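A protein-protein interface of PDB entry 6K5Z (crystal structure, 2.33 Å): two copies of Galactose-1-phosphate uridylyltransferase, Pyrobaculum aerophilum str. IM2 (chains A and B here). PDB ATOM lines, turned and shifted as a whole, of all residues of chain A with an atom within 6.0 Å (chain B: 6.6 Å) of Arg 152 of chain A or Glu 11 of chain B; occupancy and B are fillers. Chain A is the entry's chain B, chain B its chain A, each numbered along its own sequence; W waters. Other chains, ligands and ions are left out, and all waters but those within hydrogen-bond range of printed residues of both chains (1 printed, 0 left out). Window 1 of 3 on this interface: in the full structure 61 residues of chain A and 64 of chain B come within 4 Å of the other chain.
The backbone carbonyl oxygen of Leu 287 of chain B is in hydrogen-bond range of the guanidinium group of Arg 152 of chain A, at 3.2 Å. The backbone carbonyl oxygen (O) of Gly 288 of chain B sits at hydrogen-bond distance from a ring nitrogen (NE2) of His 252 of chain A, 2.7 Å away. The side-chain carboxylate (OE2) of Glu 11 of chain B lies within salt-bridge range of the guanidinium group (NH2) of Arg 152 of chain A (2.9 Å). O of Ala 289 of chain B lies within hydrogen-bond range of N of Arg 152 of chain A (3.3 Å). O of Tyr 12 of chain B is in hydrogen-bond range of N of Phe 292 of chain A (3.2 Å). The backbone carbonyl oxygen (O) of Phe 8 of chain B lies close to the backbone NH (N) of Glu 156 of chain A (3.4 Å). The side-chain amino group (NZ) of Lys 199 of chain A is in salt-bridge range of the side-chain carboxylate (OD2) of Asp 6 of chain B, 2.6 Å away. The backbone carbonyl oxygen of Ala 155 of chain A lies close to the backbone carbonyl oxygen of Phe 8 of chain B, 3.2 Å away.
OD1 of Asp 6 of chain B is in hydrogen-bond range of N of Thr 9 of chain B, 2.8 Å away. The backbone NH (N) of Glu 286 of chain B is in hydrogen-bond range of the backbone carbonyl oxygen (O) of Leu 291 of chain B, at 3.2 Å. The side-chain hydroxyl (OG1) of Thr 9 of chain B sits at hydrogen-bond distance from the side-chain carboxylate (OE1) of Glu 11 of chain B. The backbone NH of Asp 6 of chain B sits at hydrogen-bond distance from the backbone carbonyl oxygen of Glu 11 of chain B, 2.8 Å away. The side-chain carboxylate (OE1) of Glu 268 of chain A is in hydrogen-bond range of the side-chain hydroxyl (OH) of Tyr 270 of chain A (2.4 Å).
Ala 289 of chain B touches Pro 150 of chain A (O to CB, 3.5 Å). O of Ala 289 of chain B touches CD of Pro 151 of chain A (3.6 Å). CG of Pro 151 of chain A touches O of Ser 290 of chain B (3.3 Å). Leu 291 of chain B touches Pro 151 of chain A (CD2 to CD, 3.7 Å). Arg 152 of chain A touches Thr 9 of chain B. Arg 152 of chain A touches Gly 288 of chain B. Glu 11 of chain B touches Lys 199 of chain A (OE1 to CE, 3.1 Å). CA of Gly 288 of chain B touches OH of Tyr 270 of chain A, at 3.7 Å. Pro 151 of chain B touches Ser 290 of chain A (CD to O, 3.4 Å). OG of Ser 290 of chain A touches CB of Arg 152 of chain B, at 3.5 Å.
Of chain B, only Thr 9 (3.5 Å), Glu 11 (2.9 Å), Leu 287 (3.2 Å), Gly 288 (3.5 Å), Ala 289 (3.3 Å) and Ser 290 (3.7 Å) come within 4 Å of Arg 152 of chain A. Of chain A, only Arg 152 (2.9 Å), Lys 199 (3.1 Å) and Phe 292 (3.8 Å) come within 4 Å of Glu 11 of chain B. Printed residues of chain B within 4 Å of Glu 156 of chain A: Phe 8 (3.3 Å). Printed residues of chain A within 4 Å of Arg 152 of chain B: Ser 290. Of the printed residues of chain B, Lys 199 of chain A touches Asp 6 (2.6 Å), Glu 11 (3.1 Å) and Ile 13 (3.9 Å). Printed residues of chain B within 4 Å of Phe 292 of chain A: Glu 11 (3.8 Å), Tyr 12 (3.2 Å) and Ile 13 (3.5 Å). Val 149 of chain A touches none of the printed residues of chain B. Gly 10 of chain B touches none of the printed residues of chain A. The nearest residue of chain B that does not touch Arg 152 of chain A is Asp 6 of chain B (5.2 Å). The nearest residue of chain A that does not touch Glu 11 of chain B is Ser 290 of chain A (4.1 Å). The nearest printed residue of chain B that does not touch Pro 151 of chain A is Thr 9 of chain B (7.3 Å).
Printed residues of chain A that touch a printed residue of chain B: Pro 150, Pro 151, Arg 152, Ala 155, Glu 156, Lys 199, His 252, Tyr 270, Ser 290 and Phe 292. Hydrophobic or aromatic side chains of chain A that line the printed part of chain B: Pro 150, Pro 151, His 252, Tyr 270 and Phe 292. Of the 18 printed residues of chain B, 13 touch a printed residue of chain A. Printed residues of chain B that touch a printed residue of chain A: Asp 6, Phe 8, Thr 9, Glu 11, Tyr 12, Ile 13, Pro 151, Arg 152, Leu 287, Gly 288, Ala 289, Ser 290 and Leu 291. Among the printed residues, Asp or Glu carboxylates within 4 Å of a Lys or Arg side-chain nitrogen of the other chain: Arg 152 of chain A with Glu 11 of chain B (2.9 Å) and Lys 199 of chain A with Asp 6 of chain B (2.6 Å).
Pro 151 of chain A touches Ser 290 of chain B, and with the chains exchanged Ser 290 of chain A touches Pro 151 of chain B. Arg 152 of chain A touches Ser 290 of chain B, and with the chains exchanged Ser 290 of chain A touches Arg 152 of chain B. Positions printed for both chains: 151, 152 and 290. Of the 23 pairs that touch across the chains among the printed residues, 4 have their exchanged pair printed and touching as well.
Water W1 bridges NH2 of Arg 152 of chain A (2.7 Å) and O of Leu 287 of chain B (2.8 Å).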
ATOM      1  N   VAL A 149      22.360 -34.008 -17.863  1.00  0.00           N
ATOM      2  CA  VAL A 149      22.015 -32.597 -17.768  1.00  0.00           C
ATOM      3  C   VAL A 149      21.430 -32.183 -19.135  1.00  0.00           C
ATOM      4  O   VAL A 149      21.972 -32.564 -20.176  1.00  0.00           O
ATOM      5  CB  VAL A 149      23.248 -31.716 -17.467  1.00  0.00           C
ATOM      6  CG1 VAL A 149      22.887 -30.222 -17.429  1.00  0.00           C
ATOM      7  CG2 VAL A 149      23.888 -32.149 -16.154  1.00  0.00           C
ATOM      8  N   PRO A 150      20.323 -31.411 -19.129  1.00  0.00           N
ATOM      9  CA  PRO A 150      19.770 -30.966 -20.383  1.00  0.00           C
ATOM     10  C   PRO A 150      20.779 -30.125 -21.167  1.00  0.00           C
ATOM     11  O   PRO A 150      21.359 -29.182 -20.600  1.00  0.00           O
ATOM     12  CB  PRO A 150      18.558 -30.124 -19.958  1.00  0.00           C
ATOM     13  CG  PRO A 150      18.138 -30.674 -18.634  1.00  0.00           C
ATOM     14  CD  PRO A 150      19.396 -31.184 -17.995  1.00  0.00           C
ATOM     15  N   PRO A 151      20.982 -30.462 -22.466  1.00  0.00           N
ATOM     16  CA  PRO A 151      22.021 -29.801 -23.291  1.00  0.00           C
ATOM     17  C   PRO A 151      21.930 -28.304 -23.199  1.00  0.00           C
ATOM     18  O   PRO A 151      22.947 -27.659 -23.071  1.00  0.00           O
ATOM     19  CB  PRO A 151      21.704 -30.270 -24.710  1.00  0.00           C
ATOM     20  CG  PRO A 151      21.048 -31.603 -24.507  1.00  0.00           C
ATOM     21  CD  PRO A 151      20.301 -31.543 -23.213  1.00  0.00           C
ATOM     22  N   ARG A 152      20.720 -27.746 -23.177  1.00  0.00           N
ATOM     23  CA  ARG A 152      20.627 -26.311 -23.084  1.00  0.00           C
ATOM     24  C   ARG A 152      21.165 -25.841 -21.764  1.00  0.00           C
ATOM     25  O   ARG A 152      21.851 -24.852 -21.748  1.00  0.00           O
ATOM     26  CB  ARG A 152      19.220 -25.795 -23.262  1.00  0.00           C
ATOM     27  CG  ARG A 152      19.165 -24.281 -23.286  1.00  0.00           C
ATOM     28  CD  ARG A 152      17.798 -23.783 -23.710  1.00  0.00           C
ATOM     29  NE  ARG A 152      17.731 -23.692 -25.162  1.00  0.00           N
ATOM     30  CZ  ARG A 152      17.899 -22.576 -25.856  1.00  0.00           C
ATOM     31  NH1 ARG A 152      18.106 -21.403 -25.253  1.00  0.00           N
ATOM     32  NH2 ARG A 152      17.830 -22.627 -27.177  1.00  0.00           N
ATOM     33  N   VAL A 153      20.868 -26.544 -20.665  1.00  0.00           N
ATOM     34  CA  VAL A 153      21.357 -26.109 -19.359  1.00  0.00           C
ATOM     35  C   VAL A 153      22.867 -26.323 -19.298  1.00  0.00           C
ATOM     36  O   VAL A 153      23.601 -25.411 -18.895  1.00  0.00           O
ATOM     37  CB  VAL A 153      20.620 -26.767 -18.168  1.00  0.00           C
ATOM     38  CG1 VAL A 153      21.204 -26.286 -16.860  1.00  0.00           C
ATOM     39  CG2 VAL A 153      19.147 -26.400 -18.195  1.00  0.00           C
ATOM     40  N   ARG A 154      23.317 -27.498 -19.716  1.00  0.00           N
ATOM     41  CA  ARG A 154      24.744 -27.748 -19.931  1.00  0.00           C
ATOM     42  C   ARG A 154      25.483 -26.615 -20.693  1.00  0.00           C
ATOM     43  O   ARG A 154      26.599 -26.276 -20.331  1.00  0.00           O
ATOM     44  CB  ARG A 154      24.951 -29.110 -20.613  1.00  0.00           C
ATOM     45  CG  ARG A 154      26.325 -29.357 -21.255  1.00  0.00           C
ATOM     46  CD  ARG A 154      26.621 -30.856 -21.374  1.00  0.00           C
ATOM     47  NE  ARG A 154      27.041 -31.425 -20.077  1.00  0.00           N
ATOM     48  CZ  ARG A 154      26.603 -32.561 -19.503  1.00  0.00           C
ATOM     49  NH1 ARG A 154      25.696 -33.357 -20.087  1.00  0.00           N
ATOM     50  NH2 ARG A 154      27.095 -32.913 -18.311  1.00  0.00           N
ATOM     51  N   ALA A 155      24.878 -26.013 -21.716  1.00  0.00           N
ATOM     52  CA  ALA A 155      25.559 -24.910 -22.415  1.00  0.00           C
ATOM     53  C   ALA A 155      25.596 -23.669 -21.551  1.00  0.00           C
ATOM     54  O   ALA A 155      26.613 -23.023 -21.461  1.00  0.00           O
ATOM     55  CB  ALA A 155      24.935 -24.591 -23.764  1.00  0.00           C
ATOM     56  N   GLU A 156      24.480 -23.328 -20.924  1.00  0.00           N
ATOM     57  CA  GLU A 156      24.455 -22.218 -19.963  1.00  0.00           C
ATOM     58  C   GLU A 156      25.484 -22.442 -18.836  1.00  0.00           C
ATOM     59  O   GLU A 156      26.144 -21.494 -18.400  1.00  0.00           O
ATOM     60  CB  GLU A 156      23.053 -22.012 -19.376  1.00  0.00           C
ATOM     61  CG  GLU A 156      21.963 -21.718 -20.403  1.00  0.00           C
ATOM     62  CD  GLU A 156      20.694 -21.094 -19.844  1.00  0.00           C
ATOM     63  OE1 GLU A 156      20.463 -21.089 -18.604  1.00  0.00           O
ATOM     64  OE2 GLU A 156      19.890 -20.611 -20.679  1.00  0.00           O
ATOM     65  N   LEU A 157      25.633 -23.694 -18.384  1.00  0.00           N
ATOM     66  CA  LEU A 157      26.587 -24.013 -17.319  1.00  0.00           C
ATOM     67  C   LEU A 157      28.023 -23.698 -17.709  1.00  0.00           C
ATOM     68  O   LEU A 157      28.738 -23.096 -16.918  1.00  0.00           O
ATOM     69  CB  LEU A 157      26.448 -25.463 -16.855  1.00  0.00           C
ATOM     70  CG  LEU A 157      25.273 -25.671 -15.890  1.00  0.00           C
ATOM     71  CD1 LEU A 157      24.974 -27.140 -15.674  1.00  0.00           C
ATOM     72  CD2 LEU A 157      25.528 -25.005 -14.547  1.00  0.00           C
ATOM     73  N   LYS A 199      14.437 -14.268 -27.497  1.00  0.00           N
ATOM     74  CA  LYS A 199      14.326 -15.040 -28.751  1.00  0.00           C
ATOM     75  C   LYS A 199      12.907 -15.255 -29.206  1.00  0.00           C
ATOM     76  O   LYS A 199      12.674 -15.427 -30.398  1.00  0.00           O
ATOM     77  CB  LYS A 199      14.885 -16.439 -28.563  1.00  0.00           C
ATOM     78  CG  LYS A 199      16.355 -16.464 -28.474  1.00  0.00           C
ATOM     79  CD  LYS A 199      16.856 -17.770 -27.883  1.00  0.00           C
ATOM     80  CE  LYS A 199      18.146 -17.526 -27.105  1.00  0.00           C
ATOM     81  NZ  LYS A 199      17.951 -16.584 -25.963  1.00  0.00           N
ATOM     82  N   HIS A 252      15.474 -23.292 -15.069  1.00  0.00           N
ATOM     83  CA  HIS A 252      16.912 -23.507 -15.298  1.00  0.00           C
ATOM     84  C   HIS A 252      17.633 -23.337 -13.964  1.00  0.00           C
ATOM     85  O   HIS A 252      17.673 -22.243 -13.412  1.00  0.00           O
ATOM     86  CB  HIS A 252      17.468 -22.511 -16.323  1.00  0.00           C
ATOM     87  CG  HIS A 252      17.098 -22.820 -17.748  1.00  0.00           C
ATOM     88  ND1 HIS A 252      17.500 -22.025 -18.804  1.00  0.00           N
ATOM     89  CD2 HIS A 252      16.364 -23.819 -18.295  1.00  0.00           C
ATOM     90  CE1 HIS A 252      17.046 -22.531 -19.931  1.00  0.00           C
ATOM     91  NE2 HIS A 252      16.366 -23.624 -19.652  1.00  0.00           N
ATOM     92  N   TYR A 263      26.509 -20.441 -11.627  1.00  0.00           N
ATOM     93  CA  TYR A 263      25.178 -20.577 -12.203  1.00  0.00           C
ATOM     94  C   TYR A 263      24.136 -20.173 -11.176  1.00  0.00           C
ATOM     95  O   TYR A 263      24.244 -20.531 -10.007  1.00  0.00           O
ATOM     96  CB  TYR A 263      24.947 -22.019 -12.649  1.00  0.00           C
ATOM     97  CG  TYR A 263      23.852 -22.165 -13.660  1.00  0.00           C
ATOM     98  CD1 TYR A 263      23.898 -21.454 -14.857  1.00  0.00           C
ATOM     99  CD2 TYR A 263      22.750 -23.013 -13.426  1.00  0.00           C
ATOM    100  CE1 TYR A 263      22.904 -21.575 -15.793  1.00  0.00           C
ATOM    101  CE2 TYR A 263      21.733 -23.138 -14.361  1.00  0.00           C
ATOM    102  CZ  TYR A 263      21.818 -22.420 -15.541  1.00  0.00           C
ATOM    103  OH  TYR A 263      20.831 -22.541 -16.491  1.00  0.00           O
ATOM    104  N   GLU A 268      12.353 -19.437 -17.245  1.00  0.00           N
ATOM    105  CA  GLU A 268      12.177 -18.807 -18.560  1.00  0.00           C
ATOM    106  C   GLU A 268      10.793 -19.094 -19.005  1.00  0.00           C
ATOM    107  O   GLU A 268      10.330 -20.244 -18.957  1.00  0.00           O
ATOM    108  CB  GLU A 268      13.179 -19.324 -19.597  1.00  0.00           C
ATOM    109  CG  GLU A 268      14.621 -19.042 -19.195  1.00  0.00           C
ATOM    110  CD  GLU A 268      15.690 -19.293 -20.243  1.00  0.00           C
ATOM    111  OE1 GLU A 268      15.496 -20.038 -21.201  1.00  0.00           O
ATOM    112  OE2 GLU A 268      16.771 -18.708 -20.085  1.00  0.00           O
ATOM    113  N   TYR A 270       8.583 -18.568 -22.367  1.00  0.00           N
ATOM    114  CA  TYR A 270       8.443 -18.175 -23.785  1.00  0.00           C
ATOM    115  C   TYR A 270       6.977 -18.038 -24.165  1.00  0.00           C
ATOM    116  O   TYR A 270       6.284 -19.016 -24.349  1.00  0.00           O
ATOM    117  CB  TYR A 270       9.140 -19.162 -24.709  1.00  0.00           C
ATOM    118  CG  TYR A 270      10.465 -19.694 -24.208  1.00  0.00           C
ATOM    119  CD1 TYR A 270      11.365 -18.875 -23.545  1.00  0.00           C
ATOM    120  CD2 TYR A 270      10.832 -21.032 -24.447  1.00  0.00           C
ATOM    121  CE1 TYR A 270      12.586 -19.357 -23.102  1.00  0.00           C
ATOM    122  CE2 TYR A 270      12.039 -21.529 -23.985  1.00  0.00           C
ATOM    123  CZ  TYR A 270      12.918 -20.672 -23.323  1.00  0.00           C
ATOM    124  OH  TYR A 270      14.106 -21.158 -22.877  1.00  0.00           O
ATOM    125  N   SER A 290      19.041 -22.954 -35.303  1.00  0.00           N
ATOM    126  CA  SER A 290      19.082 -22.185 -34.037  1.00  0.00           C
ATOM    127  C   SER A 290      19.301 -20.687 -34.234  1.00  0.00           C
ATOM    128  O   SER A 290      20.104 -20.070 -33.535  1.00  0.00           O
ATOM    129  CB  SER A 290      20.123 -22.760 -33.049  1.00  0.00           C
ATOM    130  OG  SER A 290      19.894 -24.118 -32.793  1.00  0.00           O
ATOM    131  N   PHE A 292      17.146 -17.066 -34.424  1.00  0.00           N
ATOM    132  CA  PHE A 292      15.871 -16.492 -33.987  1.00  0.00           C
ATOM    133  C   PHE A 292      15.710 -15.134 -34.609  1.00  0.00           C
ATOM    134  O   PHE A 292      16.692 -14.510 -34.965  1.00  0.00           O
ATOM    135  CB  PHE A 292      15.817 -16.495 -32.462  1.00  0.00           C
ATOM    136  CG  PHE A 292      16.016 -17.884 -31.899  1.00  0.00           C
ATOM    137  CD1 PHE A 292      14.944 -18.781 -31.804  1.00  0.00           C
ATOM    138  CD2 PHE A 292      17.283 -18.344 -31.595  1.00  0.00           C
ATOM    139  CE1 PHE A 292      15.151 -20.083 -31.339  1.00  0.00           C
ATOM    140  CE2 PHE A 292      17.502 -19.654 -31.160  1.00  0.00           C
ATOM    141  CZ  PHE A 292      16.426 -20.526 -31.027  1.00  0.00           C
ATOM    142  N   ARG B   4      21.673  -9.751 -32.164  1.00  0.00           N
ATOM    143  CA  ARG B   4      22.074  -9.842 -30.775  1.00  0.00           C
ATOM    144  C   ARG B   4      22.534 -11.238 -30.487  1.00  0.00           C
ATOM    145  O   ARG B   4      22.299 -12.155 -31.263  1.00  0.00           O
ATOM    146  CB  ARG B   4      20.935  -9.428 -29.868  1.00  0.00           C
ATOM    147  CG  ARG B   4      20.412  -8.043 -30.206  1.00  0.00           C
ATOM    148  CD  ARG B   4      19.401  -7.551 -29.191  1.00  0.00           C
ATOM    149  NE  ARG B   4      18.835  -6.244 -29.531  1.00  0.00           N
ATOM    150  CZ  ARG B   4      18.072  -5.507 -28.715  1.00  0.00           C
ATOM    151  NH1 ARG B   4      17.761  -5.943 -27.483  1.00  0.00           N
ATOM    152  NH2 ARG B   4      17.595  -4.325 -29.134  1.00  0.00           N
ATOM    153  N   LYS B   5      23.233 -11.382 -29.380  1.00  0.00           N
ATOM    154  CA  LYS B   5      23.914 -12.622 -29.060  1.00  0.00           C
ATOM    155  C   LYS B   5      23.532 -12.993 -27.630  1.00  0.00           C
ATOM    156  O   LYS B   5      23.575 -12.163 -26.731  1.00  0.00           O
ATOM    157  CB  LYS B   5      25.414 -12.448 -29.213  1.00  0.00           C
ATOM    158  CG  LYS B   5      26.219 -13.737 -29.105  1.00  0.00           C
ATOM    159  CD  LYS B   5      27.650 -13.541 -29.627  1.00  0.00           C
ATOM    160  CE  LYS B   5      28.315 -14.850 -30.040  1.00  0.00           C
ATOM    161  NZ  LYS B   5      29.095 -15.418 -28.925  1.00  0.00           N
ATOM    162  N   ASP B   6      23.093 -14.228 -27.455  1.00  0.00           N
ATOM    163  CA  ASP B   6      22.753 -14.732 -26.165  1.00  0.00           C
ATOM    164  C   ASP B   6      24.064 -15.095 -25.498  1.00  0.00           C
ATOM    165  O   ASP B   6      24.818 -15.913 -26.013  1.00  0.00           O
ATOM    166  CB  ASP B   6      21.866 -15.954 -26.305  1.00  0.00           C
ATOM    167  CG  ASP B   6      21.446 -16.558 -24.971  1.00  0.00           C
ATOM    168  OD1 ASP B   6      22.299 -16.989 -24.163  1.00  0.00           O
ATOM    169  OD2 ASP B   6      20.231 -16.701 -24.780  1.00  0.00           O
ATOM    170  N   PRO B   7      24.338 -14.485 -24.349  1.00  0.00           N
ATOM    171  CA  PRO B   7      25.574 -14.775 -23.643  1.00  0.00           C
ATOM    172  C   PRO B   7      25.669 -16.144 -22.982  1.00  0.00           C
ATOM    173  O   PRO B   7      26.787 -16.547 -22.631  1.00  0.00           O
ATOM    174  CB  PRO B   7      25.600 -13.702 -22.577  1.00  0.00           C
ATOM    175  CG  PRO B   7      24.167 -13.389 -22.351  1.00  0.00           C
ATOM    176  CD  PRO B   7      23.610 -13.370 -23.717  1.00  0.00           C
ATOM    177  N   PHE B   8      24.543 -16.847 -22.802  1.00  0.00           N
ATOM    178  CA  PHE B   8      24.557 -18.151 -22.116  1.00  0.00           C
ATOM    179  C   PHE B   8      24.573 -19.365 -23.019  1.00  0.00           C
ATOM    180  O   PHE B   8      25.082 -20.428 -22.619  1.00  0.00           O
ATOM    181  CB  PHE B   8      23.415 -18.243 -21.098  1.00  0.00           C
ATOM    182  CG  PHE B   8      23.458 -17.136 -20.082  1.00  0.00           C
ATOM    183  CD1 PHE B   8      24.393 -17.174 -19.055  1.00  0.00           C
ATOM    184  CD2 PHE B   8      22.612 -16.016 -20.190  1.00  0.00           C
ATOM    185  CE1 PHE B   8      24.471 -16.135 -18.135  1.00  0.00           C
ATOM    186  CE2 PHE B   8      22.680 -14.980 -19.261  1.00  0.00           C
ATOM    187  CZ  PHE B   8      23.612 -15.036 -18.234  1.00  0.00           C
ATOM    188  N   THR B   9      23.990 -19.200 -24.204  1.00  0.00           N
ATOM    189  CA  THR B   9      23.805 -20.276 -25.193  1.00  0.00           C
ATOM    190  C   THR B   9      24.610 -20.085 -26.469  1.00  0.00           C
ATOM    191  O   THR B   9      24.777 -21.040 -27.205  1.00  0.00           O
ATOM    192  CB  THR B   9      22.337 -20.358 -25.630  1.00  0.00           C
ATOM    193  OG1 THR B   9      21.976 -19.107 -26.243  1.00  0.00           O
ATOM    194  CG2 THR B   9      21.414 -20.649 -24.412  1.00  0.00           C
ATOM    195  N   GLY B  10      25.060 -18.857 -26.745  1.00  0.00           N
ATOM    196  CA  GLY B  10      25.790 -18.536 -27.985  1.00  0.00           C
ATOM    197  C   GLY B  10      24.902 -18.208 -29.179  1.00  0.00           C
ATOM    198  O   GLY B  10      25.408 -17.865 -30.249  1.00  0.00           O
ATOM    199  N   GLU B  11      23.583 -18.273 -28.993  1.00  0.00           N
ATOM    200  CA  GLU B  11      22.656 -18.151 -30.097  1.00  0.00           C
ATOM    201  C   GLU B  11      22.441 -16.723 -30.549  1.00  0.00           C
ATOM    202  O   GLU B  11      22.521 -15.772 -29.742  1.00  0.00           O
ATOM    203  CB  GLU B  11      21.314 -18.764 -29.735  1.00  0.00           C
ATOM    204  CG  GLU B  11      21.404 -20.258 -29.581  1.00  0.00           C
ATOM    205  CD  GLU B  11      20.248 -20.813 -28.802  1.00  0.00           C
ATOM    206  OE1 GLU B  11      19.746 -20.117 -27.899  1.00  0.00           O
ATOM    207  OE2 GLU B  11      19.862 -21.956 -29.072  1.00  0.00           O
ATOM    208  N   TYR B  12      22.086 -16.604 -31.826  1.00  0.00           N
ATOM    209  CA  TYR B  12      21.897 -15.308 -32.444  1.00  0.00           C
ATOM    210  C   TYR B  12      20.461 -14.981 -32.592  1.00  0.00           C
ATOM    211  O   TYR B  12      19.652 -15.854 -32.866  1.00  0.00           O
ATOM    212  CB  TYR B  12      22.579 -15.236 -33.814  1.00  0.00           C
ATOM    213  CG  TYR B  12      24.094 -15.250 -33.711  1.00  0.00           C
ATOM    214  CD1 TYR B  12      24.797 -14.152 -33.191  1.00  0.00           C
ATOM    215  CD2 TYR B  12      24.814 -16.346 -34.137  1.00  0.00           C
ATOM    216  CE1 TYR B  12      26.190 -14.180 -33.100  1.00  0.00           C
ATOM    217  CE2 TYR B  12      26.188 -16.383 -34.060  1.00  0.00           C
ATOM    218  CZ  TYR B  12      26.875 -15.314 -33.537  1.00  0.00           C
ATOM    219  OH  TYR B  12      28.235 -15.403 -33.479  1.00  0.00           O
ATOM    220  N   ILE B  13      20.156 -13.697 -32.410  1.00  0.00           N
ATOM    221  CA  ILE B  13      18.828 -13.196 -32.573  1.00  0.00           C
ATOM    222  C   ILE B  13      18.865 -12.069 -33.557  1.00  0.00           C
ATOM    223  O   ILE B  13      19.516 -11.094 -33.326  1.00  0.00           O
ATOM    224  CB  ILE B  13      18.242 -12.616 -31.266  1.00  0.00           C
ATOM    225  CG1 ILE B  13      18.345 -13.591 -30.098  1.00  0.00           C
ATOM    226  CG2 ILE B  13      16.781 -12.246 -31.522  1.00  0.00           C
ATOM    227  CD1 ILE B  13      19.582 -13.439 -29.202  1.00  0.00           C
ATOM    228  N   PRO B 151      24.189 -21.045 -35.179  1.00  0.00           N
ATOM    229  CA  PRO B 151      24.696 -21.794 -34.035  1.00  0.00           C
ATOM    230  C   PRO B 151      24.515 -23.261 -34.071  1.00  0.00           C
ATOM    231  O   PRO B 151      25.345 -23.973 -33.514  1.00  0.00           O
ATOM    232  CB  PRO B 151      23.936 -21.203 -32.840  1.00  0.00           C
ATOM    233  CG  PRO B 151      23.545 -19.826 -33.284  1.00  0.00           C
ATOM    234  CD  PRO B 151      23.300 -19.941 -34.760  1.00  0.00           C
ATOM    235  N   ARG B 152      23.456 -23.758 -34.690  1.00  0.00           N
ATOM    236  CA  ARG B 152      23.311 -25.226 -34.780  1.00  0.00           C
ATOM    237  C   ARG B 152      24.349 -25.786 -35.729  1.00  0.00           C
ATOM    238  O   ARG B 152      24.883 -26.861 -35.487  1.00  0.00           O
ATOM    239  CB  ARG B 152      21.902 -25.615 -35.248  1.00  0.00           C
ATOM    240  CG  ARG B 152      21.703 -27.090 -35.575  1.00  0.00           C
ATOM    241  CD  ARG B 152      20.235 -27.403 -35.673  1.00  0.00           C
ATOM    242  NE  ARG B 152      19.662 -27.544 -34.347  1.00  0.00           N
ATOM    243  CZ  ARG B 152      19.469 -28.692 -33.699  1.00  0.00           C
ATOM    244  NH1 ARG B 152      19.736 -29.877 -34.258  1.00  0.00           N
ATOM    245  NH2 ARG B 152      18.977 -28.649 -32.464  1.00  0.00           N
ATOM    246  N   GLU B 286      11.818 -29.277 -25.548  1.00  0.00           N
ATOM    247  CA  GLU B 286      12.581 -28.929 -26.756  1.00  0.00           C
ATOM    248  C   GLU B 286      13.155 -27.517 -26.769  1.00  0.00           C
ATOM    249  O   GLU B 286      14.343 -27.340 -26.923  1.00  0.00           O
ATOM    250  CB  GLU B 286      11.743 -29.138 -28.020  1.00  0.00           C
ATOM    251  CG  GLU B 286      11.233 -30.554 -28.250  1.00  0.00           C
ATOM    252  CD  GLU B 286       9.945 -30.916 -27.499  1.00  0.00           C
ATOM    253  OE1 GLU B 286       9.292 -30.085 -26.808  1.00  0.00           O
ATOM    254  OE2 GLU B 286       9.569 -32.087 -27.611  1.00  0.00           O
ATOM    255  N   LEU B 287      12.326 -26.499 -26.648  1.00  0.00           N
ATOM    256  CA  LEU B 287      12.838 -25.106 -26.667  1.00  0.00           C
ATOM    257  C   LEU B 287      13.553 -24.744 -25.384  1.00  0.00           C
ATOM    258  O   LEU B 287      14.608 -24.108 -25.412  1.00  0.00           O
ATOM    259  CB  LEU B 287      11.700 -24.124 -26.855  1.00  0.00           C
ATOM    260  CG  LEU B 287      10.905 -24.396 -28.122  1.00  0.00           C
ATOM    261  CD1 LEU B 287       9.894 -23.270 -28.341  1.00  0.00           C
ATOM    262  CD2 LEU B 287      11.842 -24.582 -29.337  1.00  0.00           C
ATOM    263  N   GLY B 288      12.961 -25.164 -24.266  1.00  0.00           N
ATOM    264  CA  GLY B 288      13.444 -24.804 -22.927  1.00  0.00           C
ATOM    265  C   GLY B 288      14.622 -25.607 -22.426  1.00  0.00           C
ATOM    266  O   GLY B 288      15.345 -25.169 -21.564  1.00  0.00           O
ATOM    267  N   ALA B 289      14.812 -26.797 -22.945  1.00  0.00           N
ATOM    268  CA  ALA B 289      15.887 -27.613 -22.464  1.00  0.00           C
ATOM    269  C   ALA B 289      16.724 -28.317 -23.523  1.00  0.00           C
ATOM    270  O   ALA B 289      17.704 -28.995 -23.150  1.00  0.00           O
ATOM    271  CB  ALA B 289      15.313 -28.627 -21.459  1.00  0.00           C
ATOM    272  N   SER B 290      16.376 -28.160 -24.809  1.00  0.00           N
ATOM    273  CA  SER B 290      16.974 -28.935 -25.900  1.00  0.00           C
ATOM    274  C   SER B 290      16.972 -30.411 -25.567  1.00  0.00           C
ATOM    275  O   SER B 290      17.987 -31.094 -25.720  1.00  0.00           O
ATOM    276  CB  SER B 290      18.427 -28.448 -26.258  1.00  0.00           C
ATOM    277  OG  SER B 290      18.488 -27.073 -26.637  1.00  0.00           O
ATOM    278  N   LEU B 291      15.853 -30.911 -25.060  1.00  0.00           N
ATOM    279  CA  LEU B 291      15.641 -32.370 -24.945  1.00  0.00           C
ATOM    280  C   LEU B 291      14.491 -32.691 -25.838  1.00  0.00           C
ATOM    281  O   LEU B 291      13.524 -31.922 -25.887  1.00  0.00           O
ATOM    282  CB  LEU B 291      15.242 -32.817 -23.542  1.00  0.00           C
ATOM    283  CG  LEU B 291      16.250 -32.811 -22.408  1.00  0.00           C
ATOM    284  CD1 LEU B 291      15.483 -33.262 -21.175  1.00  0.00           C
ATOM    285  CD2 LEU B 291      17.415 -33.740 -22.682  1.00  0.00           C
HETATM  286  O   HOH W   1      15.144 -22.134 -27.358  1.00  0.00           O
